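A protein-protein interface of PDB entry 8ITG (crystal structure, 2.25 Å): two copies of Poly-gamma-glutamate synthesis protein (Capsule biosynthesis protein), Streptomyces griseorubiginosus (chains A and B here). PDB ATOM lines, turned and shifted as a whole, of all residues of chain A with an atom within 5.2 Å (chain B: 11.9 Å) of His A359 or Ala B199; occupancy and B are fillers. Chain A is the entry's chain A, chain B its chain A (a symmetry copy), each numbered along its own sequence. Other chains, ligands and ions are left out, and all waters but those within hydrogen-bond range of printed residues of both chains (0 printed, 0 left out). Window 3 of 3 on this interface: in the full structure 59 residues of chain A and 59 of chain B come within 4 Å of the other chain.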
ATOM      1  N   LEU A 355      18.553  -8.406  11.853  1.00  0.00           N
ATOM      2  CA  LEU A 355      17.261  -9.065  11.615  1.00  0.00           C
ATOM      3  C   LEU A 355      16.661  -8.481  10.328  1.00  0.00           C
ATOM      4  O   LEU A 355      17.397  -8.076   9.419  1.00  0.00           O
ATOM      5  CB  LEU A 355      16.376  -8.970  12.852  1.00  0.00           C
ATOM      6  CG  LEU A 355      16.981  -9.601  14.115  1.00  0.00           C
ATOM      7  CD1 LEU A 355      15.948  -9.714  15.229  1.00  0.00           C
ATOM      8  CD2 LEU A 355      17.606 -10.963  13.816  1.00  0.00           C
ATOM      9  N   PHE A 356      15.331  -8.427  10.222  1.00  0.00           N
ATOM     10  CA  PHE A 356      14.690  -8.206   8.927  1.00  0.00           C
ATOM     11  C   PHE A 356      14.666  -6.747   8.483  1.00  0.00           C
ATOM     12  O   PHE A 356      14.558  -6.489   7.280  1.00  0.00           O
ATOM     13  CB  PHE A 356      13.258  -8.742   8.953  1.00  0.00           C
ATOM     14  CG  PHE A 356      13.166 -10.198   9.285  1.00  0.00           C
ATOM     15  CD1 PHE A 356      13.612 -11.152   8.389  1.00  0.00           C
ATOM     16  CD2 PHE A 356      12.636 -10.616  10.494  1.00  0.00           C
ATOM     17  CE1 PHE A 356      13.532 -12.495   8.688  1.00  0.00           C
ATOM     18  CE2 PHE A 356      12.552 -11.958  10.798  1.00  0.00           C
ATOM     19  CZ  PHE A 356      13.001 -12.898   9.892  1.00  0.00           C
ATOM     20  N   ALA A 357      14.760  -5.797   9.412  1.00  0.00           N
ATOM     21  CA  ALA A 357      14.557  -4.393   9.060  1.00  0.00           C
ATOM     22  C   ALA A 357      15.517  -3.852   8.000  1.00  0.00           C
ATOM     23  O   ALA A 357      15.044  -3.136   7.099  1.00  0.00           O
ATOM     24  CB  ALA A 357      14.621  -3.533  10.328  1.00  0.00           C
ATOM     25  N   PRO A 358      16.831  -4.117   8.035  1.00  0.00           N
ATOM     26  CA  PRO A 358      17.734  -3.413   7.105  1.00  0.00           C
ATOM     27  C   PRO A 358      17.602  -3.830   5.647  1.00  0.00           C
ATOM     28  O   PRO A 358      18.018  -3.064   4.771  1.00  0.00           O
ATOM     29  CB  PRO A 358      19.133  -3.755   7.643  1.00  0.00           C
ATOM     30  CG  PRO A 358      18.914  -4.239   9.033  1.00  0.00           C
ATOM     31  CD  PRO A 358      17.592  -4.925   9.003  1.00  0.00           C
ATOM     32  N   HIS A 359      17.047  -5.002   5.350  1.00  0.00           N
ATOM     33  CA  HIS A 359      17.097  -5.571   4.008  1.00  0.00           C
ATOM     34  C   HIS A 359      15.744  -5.434   3.320  1.00  0.00           C
ATOM     35  O   HIS A 359      14.707  -5.773   3.900  1.00  0.00           O
ATOM     36  CB  HIS A 359      17.532  -7.034   4.070  1.00  0.00           C
ATOM     37  CG  HIS A 359      18.741  -7.259   4.925  1.00  0.00           C
ATOM     38  ND1 HIS A 359      20.019  -6.967   4.499  1.00  0.00           N
ATOM     39  CD2 HIS A 359      18.864  -7.727   6.190  1.00  0.00           C
ATOM     40  CE1 HIS A 359      20.878  -7.255   5.461  1.00  0.00           C
ATOM     41  NE2 HIS A 359      20.203  -7.717   6.497  1.00  0.00           N
ATOM     42  N   ARG A 360      15.765  -4.953   2.074  1.00  0.00           N
ATOM     43  CA  ARG A 360      14.538  -4.639   1.351  1.00  0.00           C
ATOM     44  C   ARG A 360      13.774  -5.873   0.892  1.00  0.00           C
ATOM     45  O   ARG A 360      12.564  -5.782   0.657  1.00  0.00           O
ATOM     46  CB  ARG A 360      14.854  -3.759   0.138  1.00  0.00           C
ATOM     47  CG  ARG A 360      13.664  -2.950  -0.351  1.00  0.00           C
ATOM     48  CD  ARG A 360      13.862  -2.450  -1.769  1.00  0.00           C
ATOM     49  NE  ARG A 360      12.634  -2.567  -2.549  1.00  0.00           N
ATOM     50  CZ  ARG A 360      12.279  -3.658  -3.221  1.00  0.00           C
ATOM     51  NH1 ARG A 360      13.065  -4.728  -3.211  1.00  0.00           N
ATOM     52  NH2 ARG A 360      11.144  -3.680  -3.908  1.00  0.00           N
ATOM     53  N   ARG A 361      14.442  -7.021   0.764  1.00  0.00           N
ATOM     54  CA  ARG A 361      13.757  -8.214   0.278  1.00  0.00           C
ATOM     55  C   ARG A 361      12.667  -8.670   1.239  1.00  0.00           C
ATOM     56  O   ARG A 361      11.701  -9.318   0.820  1.00  0.00           O
ATOM     57  CB  ARG A 361      14.763  -9.340   0.039  1.00  0.00           C
ATOM     58  CG  ARG A 361      15.605  -9.692   1.255  1.00  0.00           C
ATOM     59  CD  ARG A 361      16.593 -10.804   0.938  1.00  0.00           C
ATOM     60  NE  ARG A 361      17.488 -11.086   2.057  1.00  0.00           N
ATOM     61  CZ  ARG A 361      18.682 -10.524   2.222  1.00  0.00           C
ATOM     62  NH1 ARG A 361      19.130  -9.642   1.338  1.00  0.00           N
ATOM     63  NH2 ARG A 361      19.429 -10.844   3.271  1.00  0.00           N
ATOM     64  N   TYR A 362      12.794  -8.335   2.523  1.00  0.00           N
ATOM     65  CA  TYR A 362      11.815  -8.738   3.521  1.00  0.00           C
ATOM     66  C   TYR A 362      10.584  -7.841   3.559  1.00  0.00           C
ATOM     67  O   TYR A 362       9.684  -8.090   4.370  1.00  0.00           O
ATOM     68  CB  TYR A 362      12.458  -8.766   4.908  1.00  0.00           C
ATOM     69  CG  TYR A 362      13.607  -9.734   5.020  1.00  0.00           C
ATOM     70  CD1 TYR A 362      13.383 -11.104   5.053  1.00  0.00           C
ATOM     71  CD2 TYR A 362      14.914  -9.281   5.096  1.00  0.00           C
ATOM     72  CE1 TYR A 362      14.432 -11.995   5.155  1.00  0.00           C
ATOM     73  CE2 TYR A 362      15.968 -10.161   5.200  1.00  0.00           C
ATOM     74  CZ  TYR A 362      15.722 -11.515   5.229  1.00  0.00           C
ATOM     75  OH  TYR A 362      16.775 -12.391   5.334  1.00  0.00           O
ATOM     76  N   TRP A 363      10.519  -6.811   2.715  1.00  0.00           N
ATOM     77  CA  TRP A 363       9.407  -5.872   2.733  1.00  0.00           C
ATOM     78  C   TRP A 363       8.786  -5.693   1.355  1.00  0.00           C
ATOM     79  O   TRP A 363       8.023  -4.740   1.143  1.00  0.00           O
ATOM     80  CB  TRP A 363       9.866  -4.528   3.304  1.00  0.00           C
ATOM     81  CG  TRP A 363      10.609  -4.722   4.586  1.00  0.00           C
ATOM     82  CD1 TRP A 363      11.960  -4.820   4.742  1.00  0.00           C
ATOM     83  CD2 TRP A 363      10.041  -4.889   5.890  1.00  0.00           C
ATOM     84  NE1 TRP A 363      12.270  -5.021   6.064  1.00  0.00           N
ATOM     85  CE2 TRP A 363      11.110  -5.067   6.791  1.00  0.00           C
ATOM     86  CE3 TRP A 363       8.733  -4.896   6.384  1.00  0.00           C
ATOM     87  CZ2 TRP A 363      10.912  -5.247   8.158  1.00  0.00           C
ATOM     88  CZ3 TRP A 363       8.538  -5.075   7.744  1.00  0.00           C
ATOM     89  CH2 TRP A 363       9.623  -5.249   8.615  1.00  0.00           C
ATOM     90  N   PHE A 389       9.369  -0.664   3.323  1.00  0.00           N
ATOM     91  CA  PHE A 389      10.752  -0.729   3.777  1.00  0.00           C
ATOM     92  C   PHE A 389      11.252   0.657   4.173  1.00  0.00           C
ATOM     93  O   PHE A 389      11.061   1.632   3.442  1.00  0.00           O
ATOM     94  CB  PHE A 389      11.640  -1.318   2.678  1.00  0.00           C
ATOM     95  CG  PHE A 389      13.112  -1.127   2.915  1.00  0.00           C
ATOM     96  CD1 PHE A 389      13.792  -1.917   3.829  1.00  0.00           C
ATOM     97  CD2 PHE A 389      13.819  -0.162   2.215  1.00  0.00           C
ATOM     98  CE1 PHE A 389      15.148  -1.743   4.046  1.00  0.00           C
ATOM     99  CE2 PHE A 389      15.174   0.016   2.427  1.00  0.00           C
ATOM    100  CZ  PHE A 389      15.839  -0.775   3.343  1.00  0.00           C
ATOM    101  N   ARG B 191      27.387 -25.418   5.254  1.00  0.00           N
ATOM    102  CA  ARG B 191      27.691 -24.026   5.567  1.00  0.00           C
ATOM    103  C   ARG B 191      26.956 -23.074   4.633  1.00  0.00           C
ATOM    104  O   ARG B 191      26.560 -21.976   5.048  1.00  0.00           O
ATOM    105  CB  ARG B 191      29.199 -23.793   5.493  1.00  0.00           C
ATOM    106  CG  ARG B 191      29.646 -22.410   5.933  1.00  0.00           C
ATOM    107  CD  ARG B 191      31.140 -22.232   5.730  1.00  0.00           C
ATOM    108  NE  ARG B 191      31.505 -22.294   4.316  1.00  0.00           N
ATOM    109  CZ  ARG B 191      32.756 -22.365   3.870  1.00  0.00           C
ATOM    110  NH1 ARG B 191      33.769 -22.390   4.727  1.00  0.00           N
ATOM    111  NH2 ARG B 191      32.992 -22.416   2.567  1.00  0.00           N
ATOM    112  N   ALA B 192      26.758 -23.475   3.375  1.00  0.00           N
ATOM    113  CA  ALA B 192      26.056 -22.618   2.425  1.00  0.00           C
ATOM    114  C   ALA B 192      24.604 -22.404   2.827  1.00  0.00           C
ATOM    115  O   ALA B 192      24.030 -21.351   2.535  1.00  0.00           O
ATOM    116  CB  ALA B 192      26.136 -23.214   1.021  1.00  0.00           C
ATOM    117  N   ARG B 193      23.995 -23.383   3.494  1.00  0.00           N
ATOM    118  CA  ARG B 193      22.606 -23.271   3.919  1.00  0.00           C
ATOM    119  C   ARG B 193      22.429 -22.404   5.159  1.00  0.00           C
ATOM    120  O   ARG B 193      21.288 -22.193   5.586  1.00  0.00           O
ATOM    121  CB  ARG B 193      22.021 -24.666   4.159  1.00  0.00           C
ATOM    122  CG  ARG B 193      21.576 -25.334   2.870  1.00  0.00           C
ATOM    123  CD  ARG B 193      21.375 -26.828   3.013  1.00  0.00           C
ATOM    124  NE  ARG B 193      20.818 -27.395   1.786  1.00  0.00           N
ATOM    125  CZ  ARG B 193      21.528 -27.665   0.695  1.00  0.00           C
ATOM    126  NH1 ARG B 193      20.932 -28.179  -0.372  1.00  0.00           N
ATOM    127  NH2 ARG B 193      22.831 -27.421   0.668  1.00  0.00           N
ATOM    128  N   ARG B 194      23.514 -21.897   5.740  1.00  0.00           N
ATOM    129  CA  ARG B 194      23.438 -20.921   6.817  1.00  0.00           C
ATOM    130  C   ARG B 194      23.727 -19.506   6.335  1.00  0.00           C
ATOM    131  O   ARG B 194      23.901 -18.605   7.162  1.00  0.00           O
ATOM    132  CB  ARG B 194      24.402 -21.294   7.945  1.00  0.00           C
ATOM    133  CG  ARG B 194      24.160 -22.669   8.545  1.00  0.00           C
ATOM    134  CD  ARG B 194      24.927 -22.843   9.847  1.00  0.00           C
ATOM    135  NE  ARG B 194      26.355 -22.591   9.682  1.00  0.00           N
ATOM    136  CZ  ARG B 194      27.249 -23.526   9.381  1.00  0.00           C
ATOM    137  NH1 ARG B 194      26.863 -24.783   9.209  1.00  0.00           N
ATOM    138  NH2 ARG B 194      28.529 -23.205   9.251  1.00  0.00           N
ATOM    139  N   ALA B 195      23.782 -19.294   5.018  1.00  0.00           N
ATOM    140  CA  ALA B 195      24.094 -17.971   4.486  1.00  0.00           C
ATOM    141  C   ALA B 195      23.049 -16.943   4.902  1.00  0.00           C
ATOM    142  O   ALA B 195      23.383 -15.785   5.181  1.00  0.00           O
ATOM    143  CB  ALA B 195      24.207 -18.032   2.962  1.00  0.00           C
ATOM    144  N   GLU B 196      21.780 -17.348   4.950  1.00  0.00           N
ATOM    145  CA  GLU B 196      20.725 -16.437   5.385  1.00  0.00           C
ATOM    146  C   GLU B 196      20.903 -16.054   6.848  1.00  0.00           C
ATOM    147  O   GLU B 196      20.847 -14.871   7.203  1.00  0.00           O
ATOM    148  CB  GLU B 196      19.358 -17.081   5.151  1.00  0.00           C
ATOM    149  CG  GLU B 196      18.205 -16.401   5.867  1.00  0.00           C
ATOM    150  CD  GLU B 196      17.677 -15.191   5.125  1.00  0.00           C
ATOM    151  OE1 GLU B 196      18.375 -14.682   4.222  1.00  0.00           O
ATOM    152  OE2 GLU B 196      16.553 -14.751   5.445  1.00  0.00           O
ATOM    153  N   ALA B 197      21.127 -17.049   7.713  1.00  0.00           N
ATOM    154  CA  ALA B 197      21.317 -16.771   9.134  1.00  0.00           C
ATOM    155  C   ALA B 197      22.523 -15.874   9.378  1.00  0.00           C
ATOM    156  O   ALA B 197      22.557 -15.136  10.369  1.00  0.00           O
ATOM    157  CB  ALA B 197      21.469 -18.081   9.910  1.00  0.00           C
ATOM    158  N   ARG B 198      23.518 -15.921   8.489  1.00  0.00           N
ATOM    159  CA  ARG B 198      24.683 -15.058   8.633  1.00  0.00           C
ATOM    160  C   ARG B 198      24.307 -13.593   8.454  1.00  0.00           C
ATOM    161  O   ARG B 198      24.744 -12.734   9.228  1.00  0.00           O
ATOM    162  CB  ARG B 198      25.756 -15.461   7.624  1.00  0.00           C
ATOM    163  CG  ARG B 198      27.154 -15.554   8.203  1.00  0.00           C
ATOM    164  CD  ARG B 198      27.723 -16.935   7.963  1.00  0.00           C
ATOM    165  NE  ARG B 198      27.780 -17.257   6.541  1.00  0.00           N
ATOM    166  CZ  ARG B 198      27.743 -18.493   6.053  1.00  0.00           C
ATOM    167  NH1 ARG B 198      27.804 -18.691   4.744  1.00  0.00           N
ATOM    168  NH2 ARG B 198      27.633 -19.529   6.871  1.00  0.00           N
ATOM    169  N   ALA B 199      23.494 -13.287   7.440  1.00  0.00           N
ATOM    170  CA  ALA B 199      23.106 -11.903   7.191  1.00  0.00           C
ATOM    171  C   ALA B 199      22.162 -11.389   8.271  1.00  0.00           C
ATOM    172  O   ALA B 199      22.293 -10.246   8.726  1.00  0.00           O
ATOM    173  CB  ALA B 199      22.461 -11.778   5.812  1.00  0.00           C
ATOM    174  N   LEU B 200      21.209 -12.219   8.699  1.00  0.00           N
ATOM    175  CA  LEU B 200      20.229 -11.778   9.687  1.00  0.00           C
ATOM    176  C   LEU B 200      20.862 -11.596  11.062  1.00  0.00           C
ATOM    177  O   LEU B 200      20.642 -10.577  11.725  1.00  0.00           O
ATOM    178  CB  LEU B 200      19.071 -12.774   9.753  1.00  0.00           C
ATOM    179  CG  LEU B 200      18.057 -12.715   8.609  1.00  0.00           C
ATOM    180  CD1 LEU B 200      17.256 -14.005   8.536  1.00  0.00           C
ATOM    181  CD2 LEU B 200      17.127 -11.525   8.785  1.00  0.00           C
ATOM    182  N   LEU B 201      21.646 -12.580  11.514  1.00  0.00           N
ATOM    183  CA  LEU B 201      22.272 -12.488  12.828  1.00  0.00           C
ATOM    184  C   LEU B 201      23.554 -11.667  12.820  1.00  0.00           C
ATOM    185  O   LEU B 201      23.983 -11.206  13.883  1.00  0.00           O
ATOM    186  CB  LEU B 201      22.568 -13.887  13.380  1.00  0.00           C
ATOM    187  CG  LEU B 201      21.359 -14.750  13.743  1.00  0.00           C
ATOM    188  CD1 LEU B 201      21.802 -16.007  14.474  1.00  0.00           C
ATOM    189  CD2 LEU B 201      20.361 -13.959  14.578  1.00  0.00           C
ATOM    190  N   GLY B 202      24.172 -11.472  11.657  1.00  0.00           N
ATOM    191  CA  GLY B 202      25.394 -10.712  11.541  1.00  0.00           C
ATOM    192  C   GLY B 202      26.659 -11.544  11.550  1.00  0.00           C
ATOM    193  O   GLY B 202      27.715 -11.044  11.145  1.00  0.00           O
ATOM    194  N   VAL B 203      26.583 -12.798  11.993  1.00  0.00           N
ATOM    195  CA  VAL B 203      27.737 -13.684  12.086  1.00  0.00           C
ATOM    196  C   VAL B 203      27.249 -15.118  11.914  1.00  0.00           C
ATOM    197  O   VAL B 203      26.048 -15.396  11.938  1.00  0.00           O
ATOM    198  CB  VAL B 203      28.489 -13.515  13.428  1.00  0.00           C
ATOM    199  CG1 VAL B 203      27.794 -14.297  14.536  1.00  0.00           C
ATOM    200  CG2 VAL B 203      29.953 -13.919  13.290  1.00  0.00           C
ATOM    201  N   ASP B 204      28.190 -16.037  11.728  1.00  0.00           N
ATOM    202  CA  ASP B 204      27.853 -17.450  11.613  1.00  0.00           C
ATOM    203  C   ASP B 204      27.532 -18.013  12.992  1.00  0.00           C
ATOM    204  O   ASP B 204      28.398 -17.990  13.874  1.00  0.00           O
ATOM    205  CB  ASP B 204      29.005 -18.225  10.984  1.00  0.00           C
ATOM    206  CG  ASP B 204      28.569 -19.566  10.414  1.00  0.00           C
ATOM    207  OD1 ASP B 204      27.608 -20.164  10.943  1.00  0.00           O
ATOM    208  OD2 ASP B 204      29.188 -20.024   9.430  1.00  0.00           O
ATOM    209  N   PRO B 205      26.317 -18.521  13.222  1.00  0.00           N
ATOM    210  CA  PRO B 205      26.010 -19.138  14.523  1.00  0.00           C
ATOM    211  C   PRO B 205      26.811 -20.396  14.801  1.00  0.00           C
ATOM    212  O   PRO B 205      26.763 -20.902  15.929  1.00  0.00           O
ATOM    213  CB  PRO B 205      24.511 -19.447  14.422  1.00  0.00           C
ATOM    214  CG  PRO B 205      24.250 -19.560  12.957  1.00  0.00           C
ATOM    215  CD  PRO B 205      25.165 -18.563  12.305  1.00  0.00           C
ATOM    216  N   ALA B 206      27.534 -20.918  13.812  1.00  0.00           N
ATOM    217  CA  ALA B 206      28.394 -22.074  14.004  1.00  0.00           C
ATOM    218  C   ALA B 206      29.784 -21.707  14.505  1.00  0.00           C
ATOM    219  O   ALA B 206      30.521 -22.599  14.938  1.00  0.00           O
ATOM    220  CB  ALA B 206      28.513 -22.864  12.697  1.00  0.00           C
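The backbone carbonyl oxygen of Phe A356 lies within hydrogen-bond range of the indole nitrogen of Trp A363 (3.0 Å). The backbone carbonyl oxygen (O) of His A359 lies close to the indole nitrogen (NE1) of Trp A363 (3.3 Å).
Of the printed residues of chain B, Leu A355 touches Leu B200. Printed residues of chain B within 4 Å of Phe A356: Leu B200. No residue of chain B comes within 4 Å of Ala A357. No residue of chain B comes within 4 Å of Pro A358. His A359 touches just one residue of chain B: Ala B199 (3.97 Å). No residue of chain B comes within 4 Å of Arg A361. No residue of chain B comes within 4 Å of Trp A363. Of the printed residues of chain A, Glu B196 touches Tyr A362 (2.4 Å). Printed residues of chain A within 4 Å of Ala B199: His A359 (3.97 Å). Printed residues of chain A within 4 Å of Leu B200: Leu A355, Phe A356 and Tyr A362. The nearest residue of chain B that does not touch His A359 is Leu B200 (4.9 Å). The nearest printed residue of chain A that does not touch Leu B200 is His A359 (4.9 Å).
Among the printed residues, merely in contact across the chains: Tyr A362 with Leu B200 (3.5 Å), Phe A356 with Leu B200 (3.6 Å) and His A359 with Ala B199 (3.97 Å).
The backbone NH of Leu A355 lies within hydrogen-bond range of the backbone carbonyl oxygen of Leu B200, 3.0 Å away. The side-chain hydroxyl (OH) of Tyr A362 lies close to the side-chain carboxylate (OE1) of Glu B196 (3.0 Å).
Of the 16 printed residues of chain B, 3 touch a printed residue of chain A. Printed residues of chain B that touch a printed residue of chain A: Glu B196, Ala B199 and Leu B200. Hydrophobic or aromatic side chains of chain B within 4 Å of the printed part of chain A: Leu B200. Along chain B the printed residues that touch a printed residue of chain A span positions 196 to 200.
No position is printed for both chains. Of the 5 pairs that touch across the chains among the printed residues, none has its exchanged pair printed and touching as well.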
